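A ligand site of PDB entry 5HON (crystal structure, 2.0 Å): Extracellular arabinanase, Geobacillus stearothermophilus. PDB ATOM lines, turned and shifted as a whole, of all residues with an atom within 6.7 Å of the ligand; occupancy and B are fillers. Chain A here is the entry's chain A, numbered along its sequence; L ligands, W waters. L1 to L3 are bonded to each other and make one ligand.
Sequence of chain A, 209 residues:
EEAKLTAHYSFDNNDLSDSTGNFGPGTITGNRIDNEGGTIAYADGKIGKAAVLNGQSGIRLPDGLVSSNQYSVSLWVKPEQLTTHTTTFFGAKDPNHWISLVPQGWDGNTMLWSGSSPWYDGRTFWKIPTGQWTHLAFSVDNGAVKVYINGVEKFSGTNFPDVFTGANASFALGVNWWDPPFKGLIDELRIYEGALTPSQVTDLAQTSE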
ATOM      1  N   THR A  84     -37.800  32.665   7.976  1.00  0.00           N
ATOM      2  CA  THR A  84     -36.525  32.302   7.334  1.00  0.00           C
ATOM      3  C   THR A  84     -35.908  31.044   7.979  1.00  0.00           C
ATOM      4  O   THR A  84     -35.999  30.854   9.197  1.00  0.00           O
ATOM      5  CB  THR A  84     -35.535  33.506   7.377  1.00  0.00           C
ATOM      6  OG1 THR A  84     -36.078  34.603   6.623  1.00  0.00           O
ATOM      7  CG2 THR A  84     -34.199  33.136   6.775  1.00  0.00           C
ATOM      8  N   HIS A  85     -35.337  30.185   7.113  1.00  0.00           N
ATOM      9  CA  HIS A  85     -34.706  28.902   7.453  1.00  0.00           C
ATOM     10  C   HIS A  85     -35.659  27.751   7.790  1.00  0.00           C
ATOM     11  O   HIS A  85     -35.255  26.595   7.823  1.00  0.00           O
ATOM     12  CB  HIS A  85     -33.718  29.079   8.612  1.00  0.00           C
ATOM     13  CG  HIS A  85     -32.752  30.205   8.411  1.00  0.00           C
ATOM     14  ND1 HIS A  85     -31.880  30.252   7.352  1.00  0.00           N
ATOM     15  CD2 HIS A  85     -32.509  31.314   9.153  1.00  0.00           C
ATOM     16  CE1 HIS A  85     -31.159  31.350   7.429  1.00  0.00           C
ATOM     17  NE2 HIS A  85     -31.520  32.009   8.517  1.00  0.00           N
ATOM     18  N   THR A  86     -36.922  28.068   8.048  1.00  0.00           N
ATOM     19  CA  THR A  86     -37.912  27.089   8.464  1.00  0.00           C
ATOM     20  C   THR A  86     -38.142  26.022   7.394  1.00  0.00           C
ATOM     21  O   THR A  86     -38.367  26.326   6.231  1.00  0.00           O
ATOM     22  CB  THR A  86     -39.224  27.786   8.825  1.00  0.00           C
ATOM     23  OG1 THR A  86     -39.167  28.205  10.191  1.00  0.00           O
ATOM     24  CG2 THR A  86     -40.437  26.865   8.629  1.00  0.00           C
ATOM     25  N   PHE A  90     -37.159  17.567   5.892  1.00  0.00           N
ATOM     26  CA  PHE A  90     -35.941  17.588   6.691  1.00  0.00           C
ATOM     27  C   PHE A  90     -35.797  16.186   7.333  1.00  0.00           C
ATOM     28  O   PHE A  90     -36.769  15.718   7.907  1.00  0.00           O
ATOM     29  CB  PHE A  90     -36.064  18.684   7.765  1.00  0.00           C
ATOM     30  CG  PHE A  90     -34.811  18.909   8.565  1.00  0.00           C
ATOM     31  CD1 PHE A  90     -34.518  18.131   9.674  1.00  0.00           C
ATOM     32  CD2 PHE A  90     -33.915  19.911   8.209  1.00  0.00           C
ATOM     33  CE1 PHE A  90     -33.365  18.335  10.406  1.00  0.00           C
ATOM     34  CE2 PHE A  90     -32.767  20.123   8.938  1.00  0.00           C
ATOM     35  CZ  PHE A  90     -32.483  19.334  10.032  1.00  0.00           C
ATOM     36  N   PRO A  95     -27.037  17.063  13.483  1.00  0.00           N
ATOM     37  CA  PRO A  95     -27.213  18.517  13.300  1.00  0.00           C
ATOM     38  C   PRO A  95     -26.190  19.215  12.395  1.00  0.00           C
ATOM     39  O   PRO A  95     -26.343  20.407  12.128  1.00  0.00           O
ATOM     40  CB  PRO A  95     -27.092  19.056  14.731  1.00  0.00           C
ATOM     41  CG  PRO A  95     -27.529  17.931  15.582  1.00  0.00           C
ATOM     42  CD  PRO A  95     -27.001  16.702  14.915  1.00  0.00           C
ATOM     43  N   ASN A  96     -25.148  18.516  11.948  1.00  0.00           N
ATOM     44  CA  ASN A  96     -24.134  19.158  11.105  1.00  0.00           C
ATOM     45  C   ASN A  96     -24.128  18.602   9.675  1.00  0.00           C
ATOM     46  O   ASN A  96     -23.320  19.018   8.844  1.00  0.00           O
ATOM     47  CB  ASN A  96     -22.740  18.997  11.730  1.00  0.00           C
ATOM     48  CG  ASN A  96     -22.450  20.070  12.777  1.00  0.00           C
ATOM     49  OD1 ASN A  96     -23.359  20.748  13.265  1.00  0.00           O
ATOM     50  ND2 ASN A  96     -21.179  20.224  13.126  1.00  0.00           N
ATOM     51  N   TRP A  98     -27.201  17.770   7.052  1.00  0.00           N
ATOM     52  CA  TRP A  98     -28.639  17.756   6.822  1.00  0.00           C
ATOM     53  C   TRP A  98     -29.068  18.299   5.461  1.00  0.00           C
ATOM     54  O   TRP A  98     -28.317  19.000   4.797  1.00  0.00           O
ATOM     55  CB  TRP A  98     -29.350  18.548   7.914  1.00  0.00           C
ATOM     56  CG  TRP A  98     -28.694  19.861   8.217  1.00  0.00           C
ATOM     57  CD1 TRP A  98     -27.774  20.114   9.176  1.00  0.00           C
ATOM     58  CD2 TRP A  98     -28.917  21.114   7.528  1.00  0.00           C
ATOM     59  NE1 TRP A  98     -27.387  21.435   9.137  1.00  0.00           N
ATOM     60  CE2 TRP A  98     -28.079  22.073   8.133  1.00  0.00           C
ATOM     61  CE3 TRP A  98     -29.731  21.504   6.466  1.00  0.00           C
ATOM     62  CZ2 TRP A  98     -28.041  23.398   7.715  1.00  0.00           C
ATOM     63  CZ3 TRP A  98     -29.687  22.821   6.051  1.00  0.00           C
ATOM     64  CH2 TRP A  98     -28.848  23.751   6.677  1.00  0.00           C
ATOM     65  N   TRP A 106     -32.131  31.706   3.171  1.00  0.00           N
ATOM     66  CA  TRP A 106     -31.320  32.838   3.587  1.00  0.00           C
ATOM     67  C   TRP A 106     -31.263  33.959   2.545  1.00  0.00           C
ATOM     68  O   TRP A 106     -30.922  35.110   2.884  1.00  0.00           O
ATOM     69  CB  TRP A 106     -29.893  32.380   3.929  1.00  0.00           C
ATOM     70  CG  TRP A 106     -29.143  31.756   2.809  1.00  0.00           C
ATOM     71  CD1 TRP A 106     -29.037  30.426   2.533  1.00  0.00           C
ATOM     72  CD2 TRP A 106     -28.359  32.434   1.815  1.00  0.00           C
ATOM     73  NE1 TRP A 106     -28.249  30.231   1.431  1.00  0.00           N
ATOM     74  CE2 TRP A 106     -27.821  31.446   0.969  1.00  0.00           C
ATOM     75  CE3 TRP A 106     -28.069  33.776   1.550  1.00  0.00           C
ATOM     76  CZ2 TRP A 106     -27.006  31.758  -0.128  1.00  0.00           C
ATOM     77  CZ3 TRP A 106     -27.260  34.080   0.475  1.00  0.00           C
ATOM     78  CH2 TRP A 106     -26.742  33.071  -0.356  1.00  0.00           C
ATOM     79  N   MET A 111     -35.563  27.419  -1.459  1.00  0.00           N
ATOM     80  CA  MET A 111     -34.315  26.733  -1.780  1.00  0.00           C
ATOM     81  C   MET A 111     -34.217  25.350  -1.170  1.00  0.00           C
ATOM     82  O   MET A 111     -34.792  25.065  -0.127  1.00  0.00           O
ATOM     83  CB  MET A 111     -33.123  27.576  -1.332  1.00  0.00           C
ATOM     84  CG  MET A 111     -32.773  27.501   0.149  1.00  0.00           C
ATOM     85  SD  MET A 111     -31.306  28.481   0.535  1.00  0.00           S
ATOM     86  CE  MET A 111     -31.884  30.104   0.094  1.00  0.00           C
ATOM     87  N   TRP A 113     -31.798  23.304   0.726  1.00  0.00           N
ATOM     88  CA  TRP A 113     -30.658  23.708   1.530  1.00  0.00           C
ATOM     89  C   TRP A 113     -29.983  22.516   2.176  1.00  0.00           C
ATOM     90  O   TRP A 113     -30.638  21.647   2.738  1.00  0.00           O
ATOM     91  CB  TRP A 113     -31.125  24.686   2.607  1.00  0.00           C
ATOM     92  CG  TRP A 113     -30.060  25.539   3.199  1.00  0.00           C
ATOM     93  CD1 TRP A 113     -28.880  25.912   2.642  1.00  0.00           C
ATOM     94  CD2 TRP A 113     -30.120  26.154   4.489  1.00  0.00           C
ATOM     95  NE1 TRP A 113     -28.190  26.712   3.506  1.00  0.00           N
ATOM     96  CE2 TRP A 113     -28.922  26.884   4.650  1.00  0.00           C
ATOM     97  CE3 TRP A 113     -31.062  26.162   5.517  1.00  0.00           C
ATOM     98  CZ2 TRP A 113     -28.646  27.611   5.809  1.00  0.00           C
ATOM     99  CZ3 TRP A 113     -30.778  26.877   6.667  1.00  0.00           C
ATOM    100  CH2 TRP A 113     -29.584  27.593   6.800  1.00  0.00           C
ATOM    101  N   SER A 114     -28.658  22.473   2.111  1.00  0.00           N
ATOM    102  CA  SER A 114     -27.948  21.439   2.835  1.00  0.00           C
ATOM    103  C   SER A 114     -26.755  22.037   3.557  1.00  0.00           C
ATOM    104  O   SER A 114     -26.102  22.959   3.064  1.00  0.00           O
ATOM    105  CB  SER A 114     -27.507  20.321   1.896  1.00  0.00           C
ATOM    106  OG  SER A 114     -27.144  19.172   2.636  1.00  0.00           O
ATOM    107  N   GLY A 115     -26.485  21.521   4.750  1.00  0.00           N
ATOM    108  CA  GLY A 115     -25.432  22.027   5.604  1.00  0.00           C
ATOM    109  C   GLY A 115     -25.235  21.103   6.796  1.00  0.00           C
ATOM    110  O   GLY A 115     -25.842  20.044   6.875  1.00  0.00           O
ATOM    111  N   SER A 116     -24.354  21.501   7.705  1.00  0.00           N
ATOM    112  CA  SER A 116     -23.527  22.686   7.506  1.00  0.00           C
ATOM    113  C   SER A 116     -22.109  22.304   7.049  1.00  0.00           C
ATOM    114  O   SER A 116     -21.270  23.184   6.832  1.00  0.00           O
ATOM    115  CB  SER A 116     -23.476  23.525   8.782  1.00  0.00           C
ATOM    116  OG  SER A 116     -23.203  22.721   9.922  1.00  0.00           O
ATOM    117  N   TRP A 119     -21.759  23.396   3.073  1.00  0.00           N
ATOM    118  CA  TRP A 119     -22.994  24.091   2.773  1.00  0.00           C
ATOM    119  C   TRP A 119     -23.302  23.997   1.304  1.00  0.00           C
ATOM    120  O   TRP A 119     -22.445  24.250   0.463  1.00  0.00           O
ATOM    121  CG  TRP A 119     -22.518  26.499   4.803  1.00  0.00           C
ATOM    122  CD1 TRP A 119     -21.625  27.043   5.673  1.00  0.00           C
ATOM    123  CD2 TRP A 119     -23.711  26.250   5.560  1.00  0.00           C
ATOM    124  NE1 TRP A 119     -22.177  27.147   6.911  1.00  0.00           N
ATOM    125  CE2 TRP A 119     -23.461  26.676   6.871  1.00  0.00           C
ATOM    126  CE3 TRP A 119     -24.962  25.712   5.237  1.00  0.00           C
ATOM    127  CZ2 TRP A 119     -24.425  26.584   7.879  1.00  0.00           C
ATOM    128  CZ3 TRP A 119     -25.913  25.614   6.242  1.00  0.00           C
ATOM    129  CH2 TRP A 119     -25.644  26.051   7.548  1.00  0.00           C
ATOM    130  N   TYR A 120     -24.539  23.630   1.005  1.00  0.00           N
ATOM    131  CA  TYR A 120     -25.006  23.584  -0.360  1.00  0.00           C
ATOM    132  C   TYR A 120     -26.207  24.524  -0.496  1.00  0.00           C
ATOM    133  O   TYR A 120     -27.153  24.451   0.280  1.00  0.00           O
ATOM    134  CB  TYR A 120     -25.378  22.158  -0.757  1.00  0.00           C
ATOM    135  CG  TYR A 120     -25.492  21.956  -2.247  1.00  0.00           C
ATOM    136  CD1 TYR A 120     -26.633  22.336  -2.945  1.00  0.00           C
ATOM    137  CD2 TYR A 120     -24.441  21.393  -2.971  1.00  0.00           C
ATOM    138  CE1 TYR A 120     -26.729  22.154  -4.322  1.00  0.00           C
ATOM    139  CE2 TYR A 120     -24.525  21.206  -4.351  1.00  0.00           C
ATOM    140  CZ  TYR A 120     -25.672  21.579  -5.026  1.00  0.00           C
ATOM    141  OH  TYR A 120     -25.766  21.392  -6.387  1.00  0.00           O
ATOM    142  N   ASP A 121     -26.140  25.405  -1.481  1.00  0.00           N
ATOM    143  CA  ASP A 121     -27.216  26.333  -1.731  1.00  0.00           C
ATOM    144  C   ASP A 121     -27.952  25.921  -3.009  1.00  0.00           C
ATOM    145  O   ASP A 121     -27.408  26.024  -4.102  1.00  0.00           O
ATOM    146  CB  ASP A 121     -26.686  27.768  -1.826  1.00  0.00           C
ATOM    147  CG  ASP A 121     -25.977  28.195  -0.558  1.00  0.00           C
ATOM    148  OD1 ASP A 121     -26.524  27.950   0.536  1.00  0.00           O
ATOM    149  OD2 ASP A 121     -24.879  28.771  -0.636  1.00  0.00           O
ATOM    150  N   ASN A 176     -37.148  21.408  12.544  1.00  0.00           N
ATOM    151  CA  ASN A 176     -35.785  20.899  12.588  1.00  0.00           C
ATOM    152  C   ASN A 176     -35.186  21.122  13.978  1.00  0.00           C
ATOM    153  O   ASN A 176     -35.862  20.934  14.987  1.00  0.00           O
ATOM    154  CB  ASN A 176     -34.917  21.537  11.483  1.00  0.00           C
ATOM    155  CG  ASN A 176     -34.934  23.048  11.487  1.00  0.00           C
ATOM    156  OD1 ASN A 176     -35.484  23.669  12.391  1.00  0.00           O
ATOM    157  ND2 ASN A 176     -34.314  23.651  10.489  1.00  0.00           N
ATOM    158  N   TRP A 178     -33.465  24.095  14.907  1.00  0.00           N
ATOM    159  CA  TRP A 178     -33.063  25.475  15.172  1.00  0.00           C
ATOM    160  C   TRP A 178     -34.110  26.534  14.915  1.00  0.00           C
ATOM    161  O   TRP A 178     -34.076  27.594  15.545  1.00  0.00           O
ATOM    162  CB  TRP A 178     -31.811  25.835  14.338  1.00  0.00           C
ATOM    163  CG  TRP A 178     -30.737  24.791  14.307  1.00  0.00           C
ATOM    164  CD1 TRP A 178     -29.698  24.635  15.189  1.00  0.00           C
ATOM    165  CD2 TRP A 178     -30.600  23.747  13.337  1.00  0.00           C
ATOM    166  NE1 TRP A 178     -28.929  23.564  14.820  1.00  0.00           N
ATOM    167  CE2 TRP A 178     -29.450  23.003  13.692  1.00  0.00           C
ATOM    168  CE3 TRP A 178     -31.323  23.380  12.209  1.00  0.00           C
ATOM    169  CZ2 TRP A 178     -29.026  21.904  12.954  1.00  0.00           C
ATOM    170  CZ3 TRP A 178     -30.895  22.286  11.477  1.00  0.00           C
ATOM    171  CH2 TRP A 178     -29.763  21.564  11.853  1.00  0.00           C
ATOM    172  N   ASP A 179     -35.050  26.277  14.011  1.00  0.00           N
ATOM    173  CA  ASP A 179     -35.857  27.349  13.448  1.00  0.00           C
ATOM    174  C   ASP A 179     -37.344  27.254  13.762  1.00  0.00           C
ATOM    175  O   ASP A 179     -37.810  26.201  14.215  1.00  0.00           O
ATOM    176  CB  ASP A 179     -35.651  27.385  11.944  1.00  0.00           C
ATOM    177  CG  ASP A 179     -34.204  27.482  11.580  1.00  0.00           C
ATOM    178  OD1 ASP A 179     -33.606  28.551  11.789  1.00  0.00           O
ATOM    179  OD2 ASP A 179     -33.668  26.484  11.088  1.00  0.00           O
HETATM  180  O1  LIG L   1     -27.097  30.827   6.090  1.00  0.00           O
HETATM  181  C1  LIG L   1     -26.087  31.222   5.153  1.00  0.00           C
HETATM  182  C2  LIG L   1     -25.217  30.034   4.794  1.00  0.00           C
HETATM  183  O2  LIG L   1     -23.850  30.372   5.058  1.00  0.00           O
HETATM  184  C3  LIG L   1     -25.310  29.707   3.307  1.00  0.00           C
HETATM  185  O3  LIG L   1     -25.974  28.448   3.117  1.00  0.00           O
HETATM  186  C4  LIG L   1     -23.872  29.675   2.828  1.00  0.00           C
HETATM  187  O4  LIG L   1     -23.748  30.208   1.519  1.00  0.00           O
HETATM  188  C5  LIG L   1     -23.162  30.564   3.819  1.00  0.00           C
HETATM  189  O5  LIG L   1     -21.782  30.204   3.917  1.00  0.00           O
HETATM  190  O1  LG2 L   2     -27.707  29.412  10.363  1.00  0.00           O
HETATM  191  C1  LG2 L   2     -28.137  30.742  10.552  1.00  0.00           C
HETATM  192  C2  LG2 L   2     -28.290  31.294   9.158  1.00  0.00           C
HETATM  193  O2  LG2 L   2     -27.638  30.371   8.282  1.00  0.00           O
HETATM  194  C3  LG2 L   2     -27.660  32.659   9.008  1.00  0.00           C
HETATM  195  O3  LG2 L   2     -28.651  33.665   8.747  1.00  0.00           O
HETATM  196  C4  LG2 L   2     -26.706  32.511   7.835  1.00  0.00           C
HETATM  197  O4  LG2 L   2     -25.414  32.873   8.314  1.00  0.00           O
HETATM  198  C5  LG2 L   2     -26.703  31.049   7.441  1.00  0.00           C
HETATM  199  O1  LG3 L   3     -27.336  24.648  10.907  1.00  0.00           O
HETATM  200  C1  LG3 L   3     -28.728  24.939  10.815  1.00  0.00           C
HETATM  201  C2  LG3 L   3     -28.926  26.321  10.246  1.00  0.00           C
HETATM  202  O2  LG3 L   3     -27.923  27.180  10.797  1.00  0.00           O
HETATM  203  C3  LG3 L   3     -30.261  26.955  10.585  1.00  0.00           C
HETATM  204  O3  LG3 L   3     -31.229  26.670   9.568  1.00  0.00           O
HETATM  205  C4  LG3 L   3     -29.944  28.442  10.661  1.00  0.00           C
HETATM  206  O4  LG3 L   3     -30.769  29.095  11.634  1.00  0.00           O
HETATM  207  C5  LG3 L   3     -28.484  28.460  11.084  1.00  0.00           C
HETATM  208  O   HOH W   1     -22.712  29.867   7.454  1.00  0.00           O
HETATM  209  O   HOH W   2     -25.351  26.037  11.398  1.00  0.00           O
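Water W1 lies within hydrogen-bond range of O2 of LIG L1 and NE1 of Trp 119.
The backbone NH (N) of Trp 98 lies within hydrogen-bond range of the backbone carbonyl oxygen (O) of Gly 115. The side-chain hydroxyl (OG) of Ser 114 lies within hydrogen-bond range of the backbone carbonyl oxygen (O) of Trp 98 (2.5 Å). The side-chain sulfur (SD) of Met 111 lies close to the indole nitrogen (NE1) of Trp 106, 3.6 Å away. The indole nitrogen (NE1) of Trp 106 lies within hydrogen-bond range of the side-chain carboxylate (OD1) of Asp 121 (3.0 Å). The backbone NH (N) of Trp 178 is in hydrogen-bond range of the side-chain amide oxygen (OD1) of Asn 176, at 3.3 Å. The backbone carbonyl oxygen (O) of Pro 95 lies close to the indole nitrogen (NE1) of Trp 98 (3.3 Å). The side-chain carboxylate (OD2) of Asp 179 is in hydrogen-bond range of the side-chain amide nitrogen (ND2) of Asn 176 (3.0 Å).
CZ2 of Trp 98 touches O1 of LG3 L3, 3.5 Å away. CE3 of Trp 119 touches O3 of LIG L1 (3.6 Å). CE3 of Trp 178 touches C1 of LG3 L3, at 3.3 Å. Of the 19 residues printed, 8 come within 4 Å of the ligand. Along chain A the residues within 4 Å of the ligand span positions 85 to 179. The nearest printed residue that does not touch the ligand is Asn 176 (4.4 Å).
The side-chain carboxylate (OD1) of Asp 121 is in hydrogen-bond range of an oxygen (O3) of LIG L1 (2.7 Å). The side-chain carboxylate (OD2) of Asp 179 lies within hydrogen-bond range of an oxygen (O3) of LG3 L3, at 2.9 Å. The indole nitrogen of Trp 113 is in hydrogen-bond range of an oxygen (O3) of LIG L1 (2.8 Å). O3 of LIG L1 lies within hydrogen-bond range of NE1 of Trp 106 (3.3 Å). NE2 of His 85 sits at hydrogen-bond distance from O3 of LG2 L2 (3.3 Å).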
